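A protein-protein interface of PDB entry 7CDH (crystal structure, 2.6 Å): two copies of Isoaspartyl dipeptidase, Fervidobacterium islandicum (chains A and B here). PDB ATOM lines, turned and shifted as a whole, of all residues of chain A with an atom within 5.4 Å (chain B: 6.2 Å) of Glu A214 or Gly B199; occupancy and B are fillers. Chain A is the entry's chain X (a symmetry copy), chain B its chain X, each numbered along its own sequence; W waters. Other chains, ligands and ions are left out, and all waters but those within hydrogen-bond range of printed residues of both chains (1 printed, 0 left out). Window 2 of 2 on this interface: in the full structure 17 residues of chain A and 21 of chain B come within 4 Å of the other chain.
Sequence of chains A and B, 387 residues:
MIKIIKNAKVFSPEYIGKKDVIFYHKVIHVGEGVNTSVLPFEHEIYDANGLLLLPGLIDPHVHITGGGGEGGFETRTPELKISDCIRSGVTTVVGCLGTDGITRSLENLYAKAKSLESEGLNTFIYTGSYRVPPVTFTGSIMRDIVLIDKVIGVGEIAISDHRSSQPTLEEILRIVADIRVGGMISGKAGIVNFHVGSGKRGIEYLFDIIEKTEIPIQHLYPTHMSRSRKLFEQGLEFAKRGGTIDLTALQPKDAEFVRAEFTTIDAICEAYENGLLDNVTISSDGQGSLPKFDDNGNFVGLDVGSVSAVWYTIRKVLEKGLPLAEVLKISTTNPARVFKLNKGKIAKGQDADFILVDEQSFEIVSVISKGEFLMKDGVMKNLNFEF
The backbone carbonyl oxygen (O) of His B162 is in hydrogen-bond range of the guanidinium group (NE) of Arg A180, at 3.3 Å. NE2 of Gln B166 sits at hydrogen-bond distance from OE1 of Glu A214 (2.9 Å). The guanidinium group (NH2) of Arg B201 is in salt-bridge range of the side-chain carboxylate (OE2) of Glu A214 (2.7 Å). O of Asp B161 lies close to OE1 of Glu A214, 3.2 Å away.
The backbone carbonyl oxygen of Ser B160 sits close to the backbone NH of Gly B197. O of Ser B160 lies within hydrogen-bond range of N of Gly B199 (3.0 Å). OG of Ser B160 is in hydrogen-bond range of O of Gly B202. The backbone carbonyl oxygen (O) of Asp B161 sits at hydrogen-bond distance from the side-chain hydroxyl (OG) of Ser B164. The side-chain hydroxyl of Ser B164 sits at hydrogen-bond distance from the backbone NH of Gln B166 (3.0 Å). OG1 of Thr A213 is in hydrogen-bond range of O of Ile A209, 2.8 Å away.
Among the printed residues, pairs that only touch across the chains: Glu A214 with His B162 (3.3 Å), Glu A214 with Ser B160 (3.3 Å), Thr A213 with Gln B166 (3.5 Å), Lys A212 with Arg B201 (3.6 Å), Ile A215 with Gln B166 (3.8 Å), Glu A214 with Gly B199 (3.9 Å) and Thr A213 with Arg B201 (3.9 Å).
Printed residues of chain B within 4 Å of Thr A213: Gln B166 (3.5 Å) and Arg B201 (3.9 Å). Glu A214 touches just these residues of chain B: Ser B160, Asp B161, His B162, Gln B166, Gly B199 and Arg B201. Printed residues of chain A within 4 Å of Asp B161: Glu A214. Ser B164 touches none of the printed residues of chain A. Gly B199 touches just one residue of chain A: Glu A214. The nearest residue of chain B that does not touch Glu A214 is Ser B164 (4.4 Å).
Of the 7 printed residues of chain A, 5 touch a printed residue of chain B. Printed residues of chain A that touch a printed residue of chain B: Arg A180, Lys A212, Thr A213, Glu A214 and Ile A215. Hydrophobic or aromatic side chains of chain A that line the printed part of chain B: Ile A215. Along chain A the printed residues that touch a printed residue of chain B span positions 180 to 215. Hydrophobic or aromatic side chains of chain B that line the printed part of chain A: His B162. Along chain B the printed residues that touch a printed residue of chain A span positions 160 to 201. Among the printed residues, 11 pairs touch across the chains. Among the printed residues, Asp or Glu carboxylates within 4 Å of a Lys or Arg side-chain nitrogen of the other chain: Glu A214 with Arg B201.
No position is printed for both chains.
Water W1 lies within hydrogen-bond range of the side-chain hydroxyl of Ser B164 (2.6 Å), the side-chain carboxylate of Glu A214 (3.0 Å), the backbone NH of Ser B160 (3.2 Å), the backbone carbonyl oxygen of Asp B161 (3.3 Å) and the side-chain amide nitrogen of Gln B166 (3.4 Å).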
ATOM      1  N   ARG A 180      12.246   9.687  -5.710  1.00  0.00           N
ATOM      2  CA  ARG A 180      11.494  10.264  -4.573  1.00  0.00           C
ATOM      3  C   ARG A 180      10.329   9.346  -4.217  1.00  0.00           C
ATOM      4  O   ARG A 180      10.152   9.010  -3.023  1.00  0.00           O
ATOM      5  CB  ARG A 180      11.011  11.684  -4.851  1.00  0.00           C
ATOM      6  CG  ARG A 180       9.913  12.139  -3.909  1.00  0.00           C
ATOM      7  CD  ARG A 180       9.812  13.641  -3.906  1.00  0.00           C
ATOM      8  NE  ARG A 180       8.749  14.118  -3.025  1.00  0.00           N
ATOM      9  CZ  ARG A 180       8.747  14.038  -1.687  1.00  0.00           C
ATOM     10  NH1 ARG A 180       9.741  13.471  -1.028  1.00  0.00           N
ATOM     11  NH2 ARG A 180       7.733  14.525  -0.996  1.00  0.00           N
ATOM     12  N   ILE A 209      14.293  22.395 -11.041  1.00  0.00           N
ATOM     13  CA  ILE A 209      13.417  21.399 -10.361  1.00  0.00           C
ATOM     14  C   ILE A 209      12.677  22.069  -9.185  1.00  0.00           C
ATOM     15  O   ILE A 209      11.452  21.868  -9.055  1.00  0.00           O
ATOM     16  CB  ILE A 209      14.240  20.171  -9.927  1.00  0.00           C
ATOM     17  CG1 ILE A 209      14.821  19.423 -11.130  1.00  0.00           C
ATOM     18  CG2 ILE A 209      13.397  19.272  -9.060  1.00  0.00           C
ATOM     19  CD1 ILE A 209      15.995  18.538 -10.789  1.00  0.00           C
ATOM     20  N   LYS A 212      10.183  25.122 -10.329  1.00  0.00           N
ATOM     21  CA  LYS A 212       9.093  24.835 -11.296  1.00  0.00           C
ATOM     22  C   LYS A 212       8.248  23.638 -10.860  1.00  0.00           C
ATOM     23  O   LYS A 212       7.249  23.366 -11.528  1.00  0.00           O
ATOM     24  CB  LYS A 212       9.674  24.552 -12.681  1.00  0.00           C
ATOM     25  CG  LYS A 212      10.522  25.663 -13.287  1.00  0.00           C
ATOM     26  CD  LYS A 212      11.338  25.146 -14.467  1.00  0.00           C
ATOM     27  CE  LYS A 212      11.664  26.190 -15.519  1.00  0.00           C
ATOM     28  NZ  LYS A 212      11.973  25.549 -16.819  1.00  0.00           N
ATOM     29  N   THR A 213       8.619  22.927  -9.800  1.00  0.00           N
ATOM     30  CA  THR A 213       7.861  21.741  -9.340  1.00  0.00           C
ATOM     31  C   THR A 213       7.790  21.723  -7.819  1.00  0.00           C
ATOM     32  O   THR A 213       8.499  22.501  -7.173  1.00  0.00           O
ATOM     33  CB  THR A 213       8.446  20.410  -9.863  1.00  0.00           C
ATOM     34  OG1 THR A 213       9.440  19.964  -8.950  1.00  0.00           O
ATOM     35  CG2 THR A 213       9.032  20.489 -11.255  1.00  0.00           C
ATOM     36  N   GLU A 214       7.047  20.748  -7.305  1.00  0.00           N
ATOM     37  CA  GLU A 214       6.718  20.544  -5.874  1.00  0.00           C
ATOM     38  C   GLU A 214       7.796  19.657  -5.218  1.00  0.00           C
ATOM     39  O   GLU A 214       7.545  19.176  -4.085  1.00  0.00           O
ATOM     40  CB  GLU A 214       5.344  19.859  -5.781  1.00  0.00           C
ATOM     41  CG  GLU A 214       4.258  20.402  -6.727  1.00  0.00           C
ATOM     42  CD  GLU A 214       4.282  19.948  -8.193  1.00  0.00           C
ATOM     43  OE1 GLU A 214       4.983  18.950  -8.545  1.00  0.00           O
ATOM     44  OE2 GLU A 214       3.616  20.622  -9.000  1.00  0.00           O
ATOM     45  N   ILE A 215       8.910  19.381  -5.914  1.00  0.00           N
ATOM     46  CA  ILE A 215       9.910  18.369  -5.465  1.00  0.00           C
ATOM     47  C   ILE A 215      10.842  19.025  -4.456  1.00  0.00           C
ATOM     48  O   ILE A 215      11.428  20.083  -4.704  1.00  0.00           O
ATOM     49  CB  ILE A 215      10.667  17.723  -6.635  1.00  0.00           C
ATOM     50  CG1 ILE A 215       9.769  16.722  -7.371  1.00  0.00           C
ATOM     51  CG2 ILE A 215      11.926  17.068  -6.113  1.00  0.00           C
ATOM     52  CD1 ILE A 215      10.294  16.265  -8.707  1.00  0.00           C
ATOM     53  N   PRO A 216      10.902  18.472  -3.235  1.00  0.00           N
ATOM     54  CA  PRO A 216      11.702  19.071  -2.180  1.00  0.00           C
ATOM     55  C   PRO A 216      13.196  18.985  -2.519  1.00  0.00           C
ATOM     56  O   PRO A 216      13.631  17.967  -3.089  1.00  0.00           O
ATOM     57  CB  PRO A 216      11.394  18.248  -0.927  1.00  0.00           C
ATOM     58  CG  PRO A 216      10.228  17.347  -1.272  1.00  0.00           C
ATOM     59  CD  PRO A 216      10.149  17.288  -2.781  1.00  0.00           C
ATOM     60  N   ILE B 159      -1.179  15.124 -10.802  1.00  0.00           N
ATOM     61  CA  ILE B 159      -0.658  16.410 -11.351  1.00  0.00           C
ATOM     62  C   ILE B 159      -0.541  17.369 -10.176  1.00  0.00           C
ATOM     63  O   ILE B 159      -1.290  17.209  -9.202  1.00  0.00           O
ATOM     64  CB  ILE B 159      -1.608  16.935 -12.437  1.00  0.00           C
ATOM     65  CG1 ILE B 159      -3.051  16.989 -11.910  1.00  0.00           C
ATOM     66  CG2 ILE B 159      -1.498  16.066 -13.682  1.00  0.00           C
ATOM     67  CD1 ILE B 159      -3.981  17.827 -12.733  1.00  0.00           C
ATOM     68  N   SER B 160       0.350  18.331 -10.287  1.00  0.00           N
ATOM     69  CA  SER B 160       0.507  19.443  -9.327  1.00  0.00           C
ATOM     70  C   SER B 160       0.636  18.843  -7.935  1.00  0.00           C
ATOM     71  O   SER B 160      -0.094  19.261  -7.037  1.00  0.00           O
ATOM     72  CB  SER B 160      -0.639  20.409  -9.457  1.00  0.00           C
ATOM     73  OG  SER B 160      -0.758  20.889 -10.806  1.00  0.00           O
ATOM     74  N   ASP B 161       1.554  17.890  -7.778  1.00  0.00           N
ATOM     75  CA  ASP B 161       1.723  17.098  -6.529  1.00  0.00           C
ATOM     76  C   ASP B 161       3.168  16.600  -6.425  1.00  0.00           C
ATOM     77  O   ASP B 161       3.746  16.224  -7.448  1.00  0.00           O
ATOM     78  CB  ASP B 161       0.787  15.889  -6.477  1.00  0.00           C
ATOM     79  CG  ASP B 161       0.680  15.287  -5.095  1.00  0.00           C
ATOM     80  OD1 ASP B 161       1.533  14.436  -4.748  1.00  0.00           O
ATOM     81  OD2 ASP B 161      -0.225  15.718  -4.360  1.00  0.00           O
ATOM     82  N   HIS B 162       3.697  16.561  -5.210  1.00  0.00           N
ATOM     83  CA  HIS B 162       5.081  16.138  -4.914  1.00  0.00           C
ATOM     84  C   HIS B 162       5.244  14.614  -5.135  1.00  0.00           C
ATOM     85  O   HIS B 162       6.375  14.198  -5.277  1.00  0.00           O
ATOM     86  CB  HIS B 162       5.485  16.655  -3.524  1.00  0.00           C
ATOM     87  CG  HIS B 162       4.739  16.042  -2.390  1.00  0.00           C
ATOM     88  ND1 HIS B 162       3.611  16.615  -1.850  1.00  0.00           N
ATOM     89  CD2 HIS B 162       4.958  14.933  -1.670  1.00  0.00           C
ATOM     90  CE1 HIS B 162       3.175  15.886  -0.845  1.00  0.00           C
ATOM     91  NE2 HIS B 162       3.979  14.858  -0.727  1.00  0.00           N
ATOM     92  N   ARG B 163       4.171  13.831  -5.243  1.00  0.00           N
ATOM     93  CA  ARG B 163       4.212  12.368  -5.523  1.00  0.00           C
ATOM     94  C   ARG B 163       3.947  12.062  -7.008  1.00  0.00           C
ATOM     95  O   ARG B 163       3.906  10.844  -7.397  1.00  0.00           O
ATOM     96  CB  ARG B 163       3.208  11.626  -4.644  1.00  0.00           C
ATOM     97  CG  ARG B 163       3.482  11.729  -3.146  1.00  0.00           C
ATOM     98  CD  ARG B 163       2.188  11.499  -2.379  1.00  0.00           C
ATOM     99  NE  ARG B 163       1.335  12.685  -2.457  1.00  0.00           N
ATOM    100  CZ  ARG B 163       0.132  12.817  -1.898  1.00  0.00           C
ATOM    101  NH1 ARG B 163      -0.412  11.821  -1.219  1.00  0.00           N
ATOM    102  NH2 ARG B 163      -0.520  13.959  -2.028  1.00  0.00           N
ATOM    103  N   SER B 164       3.811  13.092  -7.844  1.00  0.00           N
ATOM    104  CA  SER B 164       3.552  12.907  -9.290  1.00  0.00           C
ATOM    105  C   SER B 164       4.832  12.377  -9.954  1.00  0.00           C
ATOM    106  O   SER B 164       5.906  12.411  -9.330  1.00  0.00           O
ATOM    107  CB  SER B 164       3.079  14.179  -9.923  1.00  0.00           C
ATOM    108  OG  SER B 164       4.177  14.974 -10.306  1.00  0.00           O
ATOM    109  N   GLN B 166       5.834  13.890 -12.510  1.00  0.00           N
ATOM    110  CA  GLN B 166       6.094  15.151 -13.252  1.00  0.00           C
ATOM    111  C   GLN B 166       5.757  14.934 -14.728  1.00  0.00           C
ATOM    112  O   GLN B 166       6.576  15.140 -15.607  1.00  0.00           O
ATOM    113  CB  GLN B 166       7.523  15.632 -12.998  1.00  0.00           C
ATOM    114  CG  GLN B 166       7.854  15.926 -11.535  1.00  0.00           C
ATOM    115  CD  GLN B 166       7.014  17.039 -10.926  1.00  0.00           C
ATOM    116  OE1 GLN B 166       6.632  17.997 -11.601  1.00  0.00           O
ATOM    117  NE2 GLN B 166       6.693  16.901  -9.638  1.00  0.00           N
ATOM    118  N   VAL B 196      -5.290  15.869  -7.938  1.00  0.00           N
ATOM    119  CA  VAL B 196      -4.706  17.231  -7.968  1.00  0.00           C
ATOM    120  C   VAL B 196      -4.112  17.543  -6.605  1.00  0.00           C
ATOM    121  O   VAL B 196      -4.854  17.566  -5.621  1.00  0.00           O
ATOM    122  CB  VAL B 196      -5.715  18.309  -8.379  1.00  0.00           C
ATOM    123  CG1 VAL B 196      -5.001  19.645  -8.504  1.00  0.00           C
ATOM    124  CG2 VAL B 196      -6.429  17.947  -9.669  1.00  0.00           C
ATOM    125  N   GLY B 197      -2.810  17.778  -6.572  1.00  0.00           N
ATOM    126  CA  GLY B 197      -2.107  18.127  -5.339  1.00  0.00           C
ATOM    127  C   GLY B 197      -2.229  19.611  -5.076  1.00  0.00           C
ATOM    128  O   GLY B 197      -3.129  20.234  -5.628  1.00  0.00           O
ATOM    129  N   SER B 198      -1.333  20.159  -4.269  1.00  0.00           N
ATOM    130  CA  SER B 198      -1.431  21.544  -3.771  1.00  0.00           C
ATOM    131  C   SER B 198      -0.469  22.430  -4.561  1.00  0.00           C
ATOM    132  O   SER B 198      -0.334  23.592  -4.201  1.00  0.00           O
ATOM    133  CB  SER B 198      -1.147  21.554  -2.314  1.00  0.00           C
ATOM    134  OG  SER B 198       0.052  20.845  -2.075  1.00  0.00           O
ATOM    135  N   GLY B 199       0.162  21.896  -5.611  1.00  0.00           N
ATOM    136  CA  GLY B 199       1.081  22.669  -6.457  1.00  0.00           C
ATOM    137  C   GLY B 199       0.395  23.853  -7.127  1.00  0.00           C
ATOM    138  O   GLY B 199      -0.813  23.773  -7.437  1.00  0.00           O
ATOM    139  N   LYS B 200       1.163  24.899  -7.415  1.00  0.00           N
ATOM    140  CA  LYS B 200       0.639  26.209  -7.882  1.00  0.00           C
ATOM    141  C   LYS B 200      -0.018  26.035  -9.247  1.00  0.00           C
ATOM    142  O   LYS B 200      -0.953  26.757  -9.525  1.00  0.00           O
ATOM    143  CB  LYS B 200       1.742  27.273  -7.859  1.00  0.00           C
ATOM    144  CG  LYS B 200       2.010  27.819  -6.461  1.00  0.00           C
ATOM    145  CD  LYS B 200       3.069  28.906  -6.433  1.00  0.00           C
ATOM    146  CE  LYS B 200       4.050  28.770  -5.282  1.00  0.00           C
ATOM    147  NZ  LYS B 200       5.445  28.994  -5.737  1.00  0.00           N
ATOM    148  N   ARG B 201       0.412  25.081 -10.053  1.00  0.00           N
ATOM    149  CA  ARG B 201      -0.165  24.851 -11.399  1.00  0.00           C
ATOM    150  C   ARG B 201      -1.618  24.357 -11.307  1.00  0.00           C
ATOM    151  O   ARG B 201      -2.331  24.510 -12.290  1.00  0.00           O
ATOM    152  CB  ARG B 201       0.726  23.879 -12.170  1.00  0.00           C
ATOM    153  CG  ARG B 201       2.039  24.484 -12.657  1.00  0.00           C
ATOM    154  CD  ARG B 201       2.996  23.459 -13.251  1.00  0.00           C
ATOM    155  NE  ARG B 201       3.467  22.510 -12.240  1.00  0.00           N
ATOM    156  CZ  ARG B 201       4.347  21.523 -12.440  1.00  0.00           C
ATOM    157  NH1 ARG B 201       4.887  21.352 -13.635  1.00  0.00           N
ATOM    158  NH2 ARG B 201       4.691  20.717 -11.440  1.00  0.00           N
ATOM    159  N   GLY B 202      -2.082  23.800 -10.190  1.00  0.00           N
ATOM    160  CA  GLY B 202      -3.474  23.303 -10.063  1.00  0.00           C
ATOM    161  C   GLY B 202      -3.911  22.496 -11.285  1.00  0.00           C
ATOM    162  O   GLY B 202      -3.171  21.593 -11.661  1.00  0.00           O
ATOM    163  N   ARG B 227      -9.461  21.094  -1.823  1.00  0.00           N
ATOM    164  CA  ARG B 227      -8.186  21.137  -1.056  1.00  0.00           C
ATOM    165  C   ARG B 227      -7.920  22.583  -0.597  1.00  0.00           C
ATOM    166  O   ARG B 227      -7.409  22.776   0.500  1.00  0.00           O
ATOM    167  CB  ARG B 227      -7.104  20.529  -1.951  1.00  0.00           C
ATOM    168  CG  ARG B 227      -5.670  20.721  -1.490  1.00  0.00           C
ATOM    169  CD  ARG B 227      -4.663  20.338  -2.571  1.00  0.00           C
ATOM    170  NE  ARG B 227      -4.789  18.959  -3.005  1.00  0.00           N
ATOM    171  CZ  ARG B 227      -4.418  17.902  -2.283  1.00  0.00           C
ATOM    172  NH1 ARG B 227      -4.589  16.673  -2.757  1.00  0.00           N
ATOM    173  NH2 ARG B 227      -3.909  18.071  -1.078  1.00  0.00           N
HETATM  174  O   HOH W   1       3.400  17.397 -10.511  1.00  0.00           O
